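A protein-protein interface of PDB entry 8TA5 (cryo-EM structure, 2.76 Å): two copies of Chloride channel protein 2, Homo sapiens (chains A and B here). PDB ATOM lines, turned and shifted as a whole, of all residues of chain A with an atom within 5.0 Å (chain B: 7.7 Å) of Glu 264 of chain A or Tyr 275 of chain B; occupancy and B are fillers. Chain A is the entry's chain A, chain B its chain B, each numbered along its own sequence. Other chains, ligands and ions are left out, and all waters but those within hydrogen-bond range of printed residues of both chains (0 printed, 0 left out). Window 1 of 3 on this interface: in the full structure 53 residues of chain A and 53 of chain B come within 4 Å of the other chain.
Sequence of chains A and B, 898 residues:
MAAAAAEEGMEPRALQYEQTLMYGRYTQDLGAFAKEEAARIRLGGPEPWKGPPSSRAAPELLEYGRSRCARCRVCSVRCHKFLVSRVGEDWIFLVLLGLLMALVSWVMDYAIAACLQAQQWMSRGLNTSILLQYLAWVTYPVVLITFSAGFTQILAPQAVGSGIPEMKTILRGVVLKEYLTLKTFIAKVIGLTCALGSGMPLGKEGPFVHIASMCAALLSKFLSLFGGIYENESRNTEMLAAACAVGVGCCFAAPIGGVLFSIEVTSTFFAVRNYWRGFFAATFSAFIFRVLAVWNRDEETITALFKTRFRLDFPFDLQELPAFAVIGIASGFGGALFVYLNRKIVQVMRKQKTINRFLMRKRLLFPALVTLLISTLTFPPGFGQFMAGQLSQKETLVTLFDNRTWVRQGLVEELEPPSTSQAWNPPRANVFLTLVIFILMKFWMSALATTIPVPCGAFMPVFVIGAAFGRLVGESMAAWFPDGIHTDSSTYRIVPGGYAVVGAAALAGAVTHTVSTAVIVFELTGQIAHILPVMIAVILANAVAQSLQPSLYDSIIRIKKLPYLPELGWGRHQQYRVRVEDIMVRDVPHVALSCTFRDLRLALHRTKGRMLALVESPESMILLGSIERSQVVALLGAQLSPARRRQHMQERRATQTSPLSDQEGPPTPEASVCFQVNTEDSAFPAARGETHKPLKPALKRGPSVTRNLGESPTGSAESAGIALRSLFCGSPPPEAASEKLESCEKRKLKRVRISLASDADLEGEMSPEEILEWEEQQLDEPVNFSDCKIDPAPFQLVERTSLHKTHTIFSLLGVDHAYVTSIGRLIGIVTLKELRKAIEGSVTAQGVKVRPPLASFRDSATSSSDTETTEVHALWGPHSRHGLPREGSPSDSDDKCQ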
ATOM      1  N   LEU A 260      17.193 -31.833 -35.628  1.00  0.00           N
ATOM      2  CA  LEU A 260      16.921 -31.009 -34.453  1.00  0.00           C
ATOM      3  C   LEU A 260      16.136 -29.755 -34.822  1.00  0.00           C
ATOM      4  O   LEU A 260      15.251 -29.330 -34.072  1.00  0.00           O
ATOM      5  CB  LEU A 260      18.226 -30.646 -33.748  1.00  0.00           C
ATOM      6  CG  LEU A 260      18.993 -31.823 -33.143  1.00  0.00           C
ATOM      7  CD1 LEU A 260      20.403 -31.408 -32.763  1.00  0.00           C
ATOM      8  CD2 LEU A 260      18.253 -32.392 -31.944  1.00  0.00           C
ATOM      9  N   PHE A 261      16.453 -29.142 -35.965  1.00  0.00           N
ATOM     10  CA  PHE A 261      15.700 -27.980 -36.423  1.00  0.00           C
ATOM     11  C   PHE A 261      14.262 -28.351 -36.763  1.00  0.00           C
ATOM     12  O   PHE A 261      13.330 -27.611 -36.428  1.00  0.00           O
ATOM     13  CB  PHE A 261      16.399 -27.358 -37.631  1.00  0.00           C
ATOM     14  CG  PHE A 261      15.743 -26.109 -38.139  1.00  0.00           C
ATOM     15  CD1 PHE A 261      16.042 -24.879 -37.580  1.00  0.00           C
ATOM     16  CD2 PHE A 261      14.838 -26.162 -39.186  1.00  0.00           C
ATOM     17  CE1 PHE A 261      15.445 -23.728 -38.048  1.00  0.00           C
ATOM     18  CE2 PHE A 261      14.238 -25.013 -39.657  1.00  0.00           C
ATOM     19  CZ  PHE A 261      14.541 -23.795 -39.087  1.00  0.00           C
ATOM     20  N   SER A 262      14.061 -29.495 -37.424  1.00  0.00           N
ATOM     21  CA  SER A 262      12.713 -29.907 -37.796  1.00  0.00           C
ATOM     22  C   SER A 262      11.863 -30.231 -36.575  1.00  0.00           C
ATOM     23  O   SER A 262      10.646 -30.016 -36.597  1.00  0.00           O
ATOM     24  CB  SER A 262      12.770 -31.112 -38.732  1.00  0.00           C
ATOM     25  OG  SER A 262      12.816 -32.323 -37.999  1.00  0.00           O
ATOM     26  N   ILE A 263      12.476 -30.755 -35.511  1.00  0.00           N
ATOM     27  CA  ILE A 263      11.714 -31.065 -34.303  1.00  0.00           C
ATOM     28  C   ILE A 263      11.162 -29.789 -33.675  1.00  0.00           C
ATOM     29  O   ILE A 263      10.012 -29.751 -33.219  1.00  0.00           O
ATOM     30  CB  ILE A 263      12.585 -31.859 -33.312  1.00  0.00           C
ATOM     31  CG1 ILE A 263      12.554 -33.350 -33.655  1.00  0.00           C
ATOM     32  CG2 ILE A 263      12.120 -31.644 -31.882  1.00  0.00           C
ATOM     33  CD1 ILE A 263      13.831 -34.082 -33.315  1.00  0.00           C
ATOM     34  N   GLU A 264      11.962 -28.720 -33.657  1.00  0.00           N
ATOM     35  CA  GLU A 264      11.581 -27.506 -32.944  1.00  0.00           C
ATOM     36  C   GLU A 264      10.509 -26.696 -33.660  1.00  0.00           C
ATOM     37  O   GLU A 264       9.751 -25.981 -32.997  1.00  0.00           O
ATOM     38  CB  GLU A 264      12.804 -26.621 -32.718  1.00  0.00           C
ATOM     39  CG  GLU A 264      13.831 -27.195 -31.769  1.00  0.00           C
ATOM     40  CD  GLU A 264      14.924 -26.201 -31.441  1.00  0.00           C
ATOM     41  OE1 GLU A 264      14.624 -25.179 -30.791  1.00  0.00           O
ATOM     42  OE2 GLU A 264      16.081 -26.436 -31.844  1.00  0.00           O
ATOM     43  N   VAL A 265      10.427 -26.776 -34.988  1.00  0.00           N
ATOM     44  CA  VAL A 265       9.558 -25.880 -35.742  1.00  0.00           C
ATOM     45  C   VAL A 265       8.216 -26.502 -36.117  1.00  0.00           C
ATOM     46  O   VAL A 265       7.303 -25.767 -36.523  1.00  0.00           O
ATOM     47  CB  VAL A 265      10.265 -25.369 -37.015  1.00  0.00           C
ATOM     48  CG1 VAL A 265      11.497 -24.559 -36.653  1.00  0.00           C
ATOM     49  CG2 VAL A 265      10.624 -26.529 -37.929  1.00  0.00           C
ATOM     50  N   THR A 266       8.065 -27.820 -35.997  1.00  0.00           N
ATOM     51  CA  THR A 266       6.829 -28.484 -36.383  1.00  0.00           C
ATOM     52  C   THR A 266       6.140 -29.209 -35.237  1.00  0.00           C
ATOM     53  O   THR A 266       5.140 -29.895 -35.477  1.00  0.00           O
ATOM     54  CB  THR A 266       7.088 -29.483 -37.519  1.00  0.00           C
ATOM     55  OG1 THR A 266       8.024 -30.476 -37.082  1.00  0.00           O
ATOM     56  CG2 THR A 266       7.639 -28.771 -38.745  1.00  0.00           C
ATOM     57  N   SER A 267       6.632 -29.081 -34.009  1.00  0.00           N
ATOM     58  CA  SER A 267       6.037 -29.789 -32.884  1.00  0.00           C
ATOM     59  C   SER A 267       6.477 -29.124 -31.590  1.00  0.00           C
ATOM     60  O   SER A 267       7.347 -28.251 -31.576  1.00  0.00           O
ATOM     61  CB  SER A 267       6.419 -31.273 -32.893  1.00  0.00           C
ATOM     62  OG  SER A 267       7.754 -31.458 -32.457  1.00  0.00           O
ATOM     63  N   HIS A 513      13.304 -18.651 -33.993  1.00  0.00           N
ATOM     64  CA  HIS A 513      13.073 -19.066 -32.606  1.00  0.00           C
ATOM     65  C   HIS A 513      13.561 -20.494 -32.361  1.00  0.00           C
ATOM     66  O   HIS A 513      12.872 -21.317 -31.753  1.00  0.00           O
ATOM     67  CB  HIS A 513      11.600 -18.921 -32.215  1.00  0.00           C
ATOM     68  CG  HIS A 513      11.187 -17.513 -31.917  1.00  0.00           C
ATOM     69  ND1 HIS A 513      10.100 -17.211 -31.126  1.00  0.00           N
ATOM     70  CD2 HIS A 513      11.712 -16.327 -32.303  1.00  0.00           C
ATOM     71  CE1 HIS A 513       9.974 -15.899 -31.038  1.00  0.00           C
ATOM     72  NE2 HIS A 513      10.939 -15.340 -31.743  1.00  0.00           N
ATOM     73  N   THR A 514      14.765 -20.788 -32.844  1.00  0.00           N
ATOM     74  CA  THR A 514      15.368 -22.103 -32.693  1.00  0.00           C
ATOM     75  C   THR A 514      16.780 -21.965 -32.144  1.00  0.00           C
ATOM     76  O   THR A 514      17.443 -20.944 -32.341  1.00  0.00           O
ATOM     77  CB  THR A 514      15.412 -22.863 -34.025  1.00  0.00           C
ATOM     78  OG1 THR A 514      15.798 -21.969 -35.075  1.00  0.00           O
ATOM     79  CG2 THR A 514      14.051 -23.452 -34.344  1.00  0.00           C
ATOM     80  N   VAL A 515      17.231 -23.007 -31.447  1.00  0.00           N
ATOM     81  CA  VAL A 515      18.596 -23.081 -30.941  1.00  0.00           C
ATOM     82  C   VAL A 515      19.417 -24.141 -31.650  1.00  0.00           C
ATOM     83  O   VAL A 515      20.573 -24.371 -31.266  1.00  0.00           O
ATOM     84  CB  VAL A 515      18.621 -23.314 -29.419  1.00  0.00           C
ATOM     85  CG1 VAL A 515      18.028 -22.122 -28.689  1.00  0.00           C
ATOM     86  CG2 VAL A 515      17.876 -24.581 -29.063  1.00  0.00           C
ATOM     87  N   SER A 516      18.866 -24.794 -32.668  1.00  0.00           N
ATOM     88  CA  SER A 516      19.593 -25.783 -33.450  1.00  0.00           C
ATOM     89  C   SER A 516      20.412 -25.160 -34.570  1.00  0.00           C
ATOM     90  O   SER A 516      21.147 -25.879 -35.257  1.00  0.00           O
ATOM     91  CB  SER A 516      18.624 -26.813 -34.034  1.00  0.00           C
ATOM     92  OG  SER A 516      17.804 -27.367 -33.023  1.00  0.00           O
ATOM     93  N   ALA B 241      14.782 -31.882 -14.496  1.00  0.00           N
ATOM     94  CA  ALA B 241      15.234 -32.214 -15.846  1.00  0.00           C
ATOM     95  C   ALA B 241      16.381 -31.308 -16.283  1.00  0.00           C
ATOM     96  O   ALA B 241      17.378 -31.773 -16.860  1.00  0.00           O
ATOM     97  CB  ALA B 241      14.068 -32.119 -16.830  1.00  0.00           C
ATOM     98  N   ALA B 245      20.310 -32.326 -17.277  1.00  0.00           N
ATOM     99  CA  ALA B 245      21.041 -31.842 -18.447  1.00  0.00           C
ATOM    100  C   ALA B 245      22.352 -31.177 -18.044  1.00  0.00           C
ATOM    101  O   ALA B 245      23.398 -31.417 -18.662  1.00  0.00           O
ATOM    102  CB  ALA B 245      20.171 -30.876 -19.249  1.00  0.00           C
ATOM    103  N   PRO B 255      28.190 -29.382 -23.686  1.00  0.00           N
ATOM    104  CA  PRO B 255      26.875 -28.825 -23.338  1.00  0.00           C
ATOM    105  C   PRO B 255      25.727 -29.327 -24.204  1.00  0.00           C
ATOM    106  O   PRO B 255      24.756 -29.877 -23.677  1.00  0.00           O
ATOM    107  CB  PRO B 255      27.086 -27.316 -23.513  1.00  0.00           C
ATOM    108  CG  PRO B 255      28.559 -27.130 -23.321  1.00  0.00           C
ATOM    109  CD  PRO B 255      29.173 -28.325 -23.974  1.00  0.00           C
ATOM    110  N   ILE B 256      25.816 -29.144 -25.523  1.00  0.00           N
ATOM    111  CA  ILE B 256      24.728 -29.561 -26.405  1.00  0.00           C
ATOM    112  C   ILE B 256      24.574 -31.076 -26.385  1.00  0.00           C
ATOM    113  O   ILE B 256      23.461 -31.606 -26.260  1.00  0.00           O
ATOM    114  CB  ILE B 256      24.962 -29.038 -27.833  1.00  0.00           C
ATOM    115  CG1 ILE B 256      25.205 -27.529 -27.814  1.00  0.00           C
ATOM    116  CG2 ILE B 256      23.780 -29.381 -28.725  1.00  0.00           C
ATOM    117  CD1 ILE B 256      25.482 -26.941 -29.177  1.00  0.00           C
ATOM    118  N   GLY B 257      25.691 -31.794 -26.516  1.00  0.00           N
ATOM    119  CA  GLY B 257      25.638 -33.243 -26.432  1.00  0.00           C
ATOM    120  C   GLY B 257      25.134 -33.722 -25.087  1.00  0.00           C
ATOM    121  O   GLY B 257      24.390 -34.700 -25.006  1.00  0.00           O
ATOM    122  N   VAL B 259      22.997 -32.110 -23.058  1.00  0.00           N
ATOM    123  CA  VAL B 259      21.554 -31.884 -22.999  1.00  0.00           C
ATOM    124  C   VAL B 259      20.818 -32.942 -23.810  1.00  0.00           C
ATOM    125  O   VAL B 259      19.828 -33.529 -23.350  1.00  0.00           O
ATOM    126  CB  VAL B 259      21.210 -30.464 -23.480  1.00  0.00           C
ATOM    127  CG1 VAL B 259      19.705 -30.275 -23.534  1.00  0.00           C
ATOM    128  CG2 VAL B 259      21.836 -29.428 -22.562  1.00  0.00           C
ATOM    129  N   LEU B 260      21.297 -33.213 -25.028  1.00  0.00           N
ATOM    130  CA  LEU B 260      20.629 -34.199 -25.872  1.00  0.00           C
ATOM    131  C   LEU B 260      20.691 -35.593 -25.258  1.00  0.00           C
ATOM    132  O   LEU B 260      19.727 -36.362 -25.349  1.00  0.00           O
ATOM    133  CB  LEU B 260      21.242 -34.200 -27.273  1.00  0.00           C
ATOM    134  CG  LEU B 260      21.114 -32.895 -28.057  1.00  0.00           C
ATOM    135  CD1 LEU B 260      21.877 -32.981 -29.367  1.00  0.00           C
ATOM    136  CD2 LEU B 260      19.654 -32.561 -28.302  1.00  0.00           C
ATOM    137  N   ILE B 263      18.152 -35.693 -22.273  1.00  0.00           N
ATOM    138  CA  ILE B 263      16.766 -35.804 -22.721  1.00  0.00           C
ATOM    139  C   ILE B 263      16.446 -37.228 -23.157  1.00  0.00           C
ATOM    140  O   ILE B 263      15.324 -37.711 -22.960  1.00  0.00           O
ATOM    141  CB  ILE B 263      16.487 -34.792 -23.851  1.00  0.00           C
ATOM    142  CG1 ILE B 263      16.670 -33.361 -23.349  1.00  0.00           C
ATOM    143  CG2 ILE B 263      15.085 -34.969 -24.408  1.00  0.00           C
ATOM    144  CD1 ILE B 263      16.311 -32.311 -24.371  1.00  0.00           C
ATOM    145  N   PHE B 270      10.184 -35.284 -25.983  1.00  0.00           N
ATOM    146  CA  PHE B 270      11.118 -34.209 -26.312  1.00  0.00           C
ATOM    147  C   PHE B 270      10.374 -32.890 -26.155  1.00  0.00           C
ATOM    148  O   PHE B 270       9.745 -32.391 -27.087  1.00  0.00           O
ATOM    149  CB  PHE B 270      11.672 -34.387 -27.722  1.00  0.00           C
ATOM    150  CG  PHE B 270      12.914 -33.585 -28.000  1.00  0.00           C
ATOM    151  CD1 PHE B 270      12.872 -32.200 -28.041  1.00  0.00           C
ATOM    152  CD2 PHE B 270      14.125 -34.219 -28.228  1.00  0.00           C
ATOM    153  CE1 PHE B 270      14.012 -31.465 -28.299  1.00  0.00           C
ATOM    154  CE2 PHE B 270      15.267 -33.487 -28.487  1.00  0.00           C
ATOM    155  CZ  PHE B 270      15.210 -32.109 -28.522  1.00  0.00           C
ATOM    156  N   ALA B 271      10.445 -32.320 -24.955  1.00  0.00           N
ATOM    157  CA  ALA B 271       9.845 -31.022 -24.682  1.00  0.00           C
ATOM    158  C   ALA B 271      10.810 -29.925 -25.109  1.00  0.00           C
ATOM    159  O   ALA B 271      11.975 -29.922 -24.701  1.00  0.00           O
ATOM    160  CB  ALA B 271       9.496 -30.883 -23.200  1.00  0.00           C
ATOM    161  N   VAL B 272      10.319 -28.996 -25.929  1.00  0.00           N
ATOM    162  CA  VAL B 272      11.193 -27.980 -26.509  1.00  0.00           C
ATOM    163  C   VAL B 272      11.674 -27.003 -25.442  1.00  0.00           C
ATOM    164  O   VAL B 272      12.832 -26.567 -25.458  1.00  0.00           O
ATOM    165  CB  VAL B 272      10.474 -27.262 -27.664  1.00  0.00           C
ATOM    166  CG1 VAL B 272      11.430 -26.337 -28.388  1.00  0.00           C
ATOM    167  CG2 VAL B 272       9.885 -28.276 -28.629  1.00  0.00           C
ATOM    168  N   ARG B 273      10.799 -26.636 -24.503  1.00  0.00           N
ATOM    169  CA  ARG B 273      11.195 -25.688 -23.465  1.00  0.00           C
ATOM    170  C   ARG B 273      12.209 -26.297 -22.502  1.00  0.00           C
ATOM    171  O   ARG B 273      13.093 -25.588 -22.005  1.00  0.00           O
ATOM    172  CB  ARG B 273       9.958 -25.180 -22.722  1.00  0.00           C
ATOM    173  CG  ARG B 273       9.281 -26.196 -21.820  1.00  0.00           C
ATOM    174  CD  ARG B 273       8.237 -25.528 -20.943  1.00  0.00           C
ATOM    175  NE  ARG B 273       7.668 -24.350 -21.588  1.00  0.00           N
ATOM    176  CZ  ARG B 273       7.398 -23.210 -20.968  1.00  0.00           C
ATOM    177  NH1 ARG B 273       7.627 -23.056 -19.674  1.00  0.00           N
ATOM    178  NH2 ARG B 273       6.885 -22.199 -21.663  1.00  0.00           N
ATOM    179  N   ASN B 274      12.110 -27.602 -22.237  1.00  0.00           N
ATOM    180  CA  ASN B 274      13.150 -28.286 -21.476  1.00  0.00           C
ATOM    181  C   ASN B 274      14.484 -28.215 -22.206  1.00  0.00           C
ATOM    182  O   ASN B 274      15.531 -27.980 -21.590  1.00  0.00           O
ATOM    183  CB  ASN B 274      12.735 -29.739 -21.231  1.00  0.00           C
ATOM    184  CG  ASN B 274      13.890 -30.620 -20.792  1.00  0.00           C
ATOM    185  OD1 ASN B 274      14.775 -30.190 -20.053  1.00  0.00           O
ATOM    186  ND2 ASN B 274      13.883 -31.867 -21.247  1.00  0.00           N
ATOM    187  N   TYR B 275      14.458 -28.408 -23.527  1.00  0.00           N
ATOM    188  CA  TYR B 275      15.661 -28.278 -24.338  1.00  0.00           C
ATOM    189  C   TYR B 275      16.254 -26.879 -24.220  1.00  0.00           C
ATOM    190  O   TYR B 275      17.468 -26.723 -24.052  1.00  0.00           O
ATOM    191  CB  TYR B 275      15.326 -28.614 -25.792  1.00  0.00           C
ATOM    192  CG  TYR B 275      16.480 -28.542 -26.767  1.00  0.00           C
ATOM    193  CD1 TYR B 275      17.766 -28.905 -26.390  1.00  0.00           C
ATOM    194  CD2 TYR B 275      16.274 -28.127 -28.076  1.00  0.00           C
ATOM    195  CE1 TYR B 275      18.815 -28.843 -27.289  1.00  0.00           C
ATOM    196  CE2 TYR B 275      17.314 -28.065 -28.979  1.00  0.00           C
ATOM    197  CZ  TYR B 275      18.582 -28.423 -28.581  1.00  0.00           C
ATOM    198  OH  TYR B 275      19.619 -28.360 -29.480  1.00  0.00           O
ATOM    199  N   TRP B 276      15.407 -25.848 -24.288  1.00  0.00           N
ATOM    200  CA  TRP B 276      15.895 -24.475 -24.191  1.00  0.00           C
ATOM    201  C   TRP B 276      16.502 -24.186 -22.821  1.00  0.00           C
ATOM    202  O   TRP B 276      17.559 -23.548 -22.724  1.00  0.00           O
ATOM    203  CB  TRP B 276      14.759 -23.497 -24.488  1.00  0.00           C
ATOM    204  CG  TRP B 276      14.264 -23.547 -25.902  1.00  0.00           C
ATOM    205  CD1 TRP B 276      14.878 -24.138 -26.967  1.00  0.00           C
ATOM    206  CD2 TRP B 276      13.045 -22.985 -26.403  1.00  0.00           C
ATOM    207  NE1 TRP B 276      14.118 -23.975 -28.100  1.00  0.00           N
ATOM    208  CE2 TRP B 276      12.989 -23.271 -27.780  1.00  0.00           C
ATOM    209  CE3 TRP B 276      11.998 -22.266 -25.819  1.00  0.00           C
ATOM    210  CZ2 TRP B 276      11.926 -22.863 -28.583  1.00  0.00           C
ATOM    211  CZ3 TRP B 276      10.944 -21.864 -26.617  1.00  0.00           C
ATOM    212  CH2 TRP B 276      10.915 -22.164 -27.984  1.00  0.00           C
ATOM    213  N   ARG B 277      15.844 -24.638 -21.749  1.00  0.00           N
ATOM    214  CA  ARG B 277      16.363 -24.393 -20.405  1.00  0.00           C
ATOM    215  C   ARG B 277      17.690 -25.113 -20.185  1.00  0.00           C
ATOM    216  O   ARG B 277      18.628 -24.540 -19.608  1.00  0.00           O
ATOM    217  CB  ARG B 277      15.333 -24.827 -19.362  1.00  0.00           C
ATOM    218  CG  ARG B 277      14.327 -23.745 -19.002  1.00  0.00           C
ATOM    219  CD  ARG B 277      13.482 -24.141 -17.803  1.00  0.00           C
ATOM    220  NE  ARG B 277      12.713 -25.354 -18.050  1.00  0.00           N
ATOM    221  CZ  ARG B 277      11.412 -25.379 -18.305  1.00  0.00           C
ATOM    222  NH1 ARG B 277      10.696 -24.267 -18.349  1.00  0.00           N
ATOM    223  NH2 ARG B 277      10.815 -26.547 -18.522  1.00  0.00           N
ATOM    224  N   GLY B 278      17.787 -26.366 -20.634  1.00  0.00           N
ATOM    225  CA  GLY B 278      19.052 -27.071 -20.551  1.00  0.00           C
ATOM    226  C   GLY B 278      20.144 -26.391 -21.353  1.00  0.00           C
ATOM    227  O   GLY B 278      21.289 -26.305 -20.907  1.00  0.00           O
ATOM    228  N   PHE B 279      19.800 -25.893 -22.543  1.00  0.00           N
ATOM    229  CA  PHE B 279      20.758 -25.156 -23.360  1.00  0.00           C
ATOM    230  C   PHE B 279      21.290 -23.938 -22.615  1.00  0.00           C
ATOM    231  O   PHE B 279      22.503 -23.707 -22.562  1.00  0.00           O
ATOM    232  CB  PHE B 279      20.086 -24.741 -24.671  1.00  0.00           C
ATOM    233  CG  PHE B 279      21.043 -24.428 -25.784  1.00  0.00           C
ATOM    234  CD1 PHE B 279      21.616 -23.173 -25.892  1.00  0.00           C
ATOM    235  CD2 PHE B 279      21.351 -25.382 -26.738  1.00  0.00           C
ATOM    236  CE1 PHE B 279      22.488 -22.879 -26.922  1.00  0.00           C
ATOM    237  CE2 PHE B 279      22.223 -25.094 -27.770  1.00  0.00           C
ATOM    238  CZ  PHE B 279      22.792 -23.840 -27.861  1.00  0.00           C
ATOM    239  N   PHE B 280      20.387 -23.161 -22.012  1.00  0.00           N
ATOM    240  CA  PHE B 280      20.788 -21.963 -21.279  1.00  0.00           C
ATOM    241  C   PHE B 280      21.726 -22.306 -20.123  1.00  0.00           C
ATOM    242  O   PHE B 280      22.812 -21.718 -19.980  1.00  0.00           O
ATOM    243  CB  PHE B 280      19.534 -21.242 -20.775  1.00  0.00           C
ATOM    244  CG  PHE B 280      19.808 -19.967 -20.032  1.00  0.00           C
ATOM    245  CD1 PHE B 280      19.809 -18.752 -20.695  1.00  0.00           C
ATOM    246  CD2 PHE B 280      20.023 -19.977 -18.664  1.00  0.00           C
ATOM    247  CE1 PHE B 280      20.049 -17.577 -20.014  1.00  0.00           C
ATOM    248  CE2 PHE B 280      20.262 -18.803 -17.978  1.00  0.00           C
ATOM    249  CZ  PHE B 280      20.275 -17.602 -18.653  1.00  0.00           C
ATOM    250  N   ALA B 281      21.321 -23.264 -19.287  1.00  0.00           N
ATOM    251  CA  ALA B 281      22.119 -23.584 -18.107  1.00  0.00           C
ATOM    252  C   ALA B 281      23.462 -24.205 -18.487  1.00  0.00           C
ATOM    253  O   ALA B 281      24.489 -23.906 -17.863  1.00  0.00           O
ATOM    254  CB  ALA B 281      21.329 -24.504 -17.182  1.00  0.00           C
ATOM    255  N   ALA B 282      23.480 -25.060 -19.514  1.00  0.00           N
ATOM    256  CA  ALA B 282      24.736 -25.654 -19.959  1.00  0.00           C
ATOM    257  C   ALA B 282      25.660 -24.604 -20.560  1.00  0.00           C
ATOM    258  O   ALA B 282      26.883 -24.691 -20.406  1.00  0.00           O
ATOM    259  CB  ALA B 282      24.462 -26.771 -20.964  1.00  0.00           C
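Among the printed residues, merely in contact across the chains: Leu 260 of chain A with Leu 260 of chain B, Ile 263 of chain A with Phe 270 of chain B, Glu 264 of chain A with Tyr 275 of chain B, Ser 267 of chain A with Val 272 of chain B, His 513 of chain A with Trp 276 of chain B, Val 515 of chain A with Tyr 275 of chain B, Val 515 of chain A with Trp 276 of chain B and Val 515 of chain A with Phe 279 of chain B.
OG of Ser 516 of chain A sits close to O of Leu 260 of chain A (3.4 Å). O of Ile 263 of chain A is in hydrogen-bond range of OG of Ser 267 of chain A, at 2.9 Å. The backbone NH (N) of Val 515 of chain A is in hydrogen-bond range of the side-chain carboxylate (OE1) of Glu 264 of chain A. OE2 of Glu 264 of chain A lies within hydrogen-bond range of N of Ser 516 of chain A, at 3.3 Å.
The indole nitrogen (NE1) of Trp 276 of chain B lies within hydrogen-bond range of the side-chain carboxylate (OE1) of Glu 264 of chain A.
Printed residues of chain A that touch a printed residue of chain B: Leu 260, Ile 263, Glu 264, Ser 267, His 513 and Val 515. Among the printed residues, 9 pairs touch across the chains.
Leu 260 of chain A touches its own counterpart, Leu 260 of chain B. 2 positions are printed for both chains. Of the 9 pairs that touch across the chains among the printed residues, 1 has its exchanged pair printed and touching as well.
Of chain B, only Tyr 275 and Trp 276 come within 4 Å of Glu 264 of chain A. Of chain A, only Glu 264 and Val 515 come within 4 Å of Tyr 275 of chain B. Printed residues of chain A within 4 Å of Phe 279 of chain B: Val 515 (3.9 Å). Of the printed residues of chain A, Val 272 of chain B touches Ser 267 (3.9 Å). Of the printed residues of chain B, Leu 260 of chain A touches Leu 260 (3.9 Å). Of the printed residues of chain A, Trp 276 of chain B touches Glu 264 (3.0 Å), His 513 (3.7 Å) and Val 515 (3.7 Å). The nearest residue of chain A that does not touch Tyr 275 of chain B is Ser 516 of chain A (4.1 Å).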
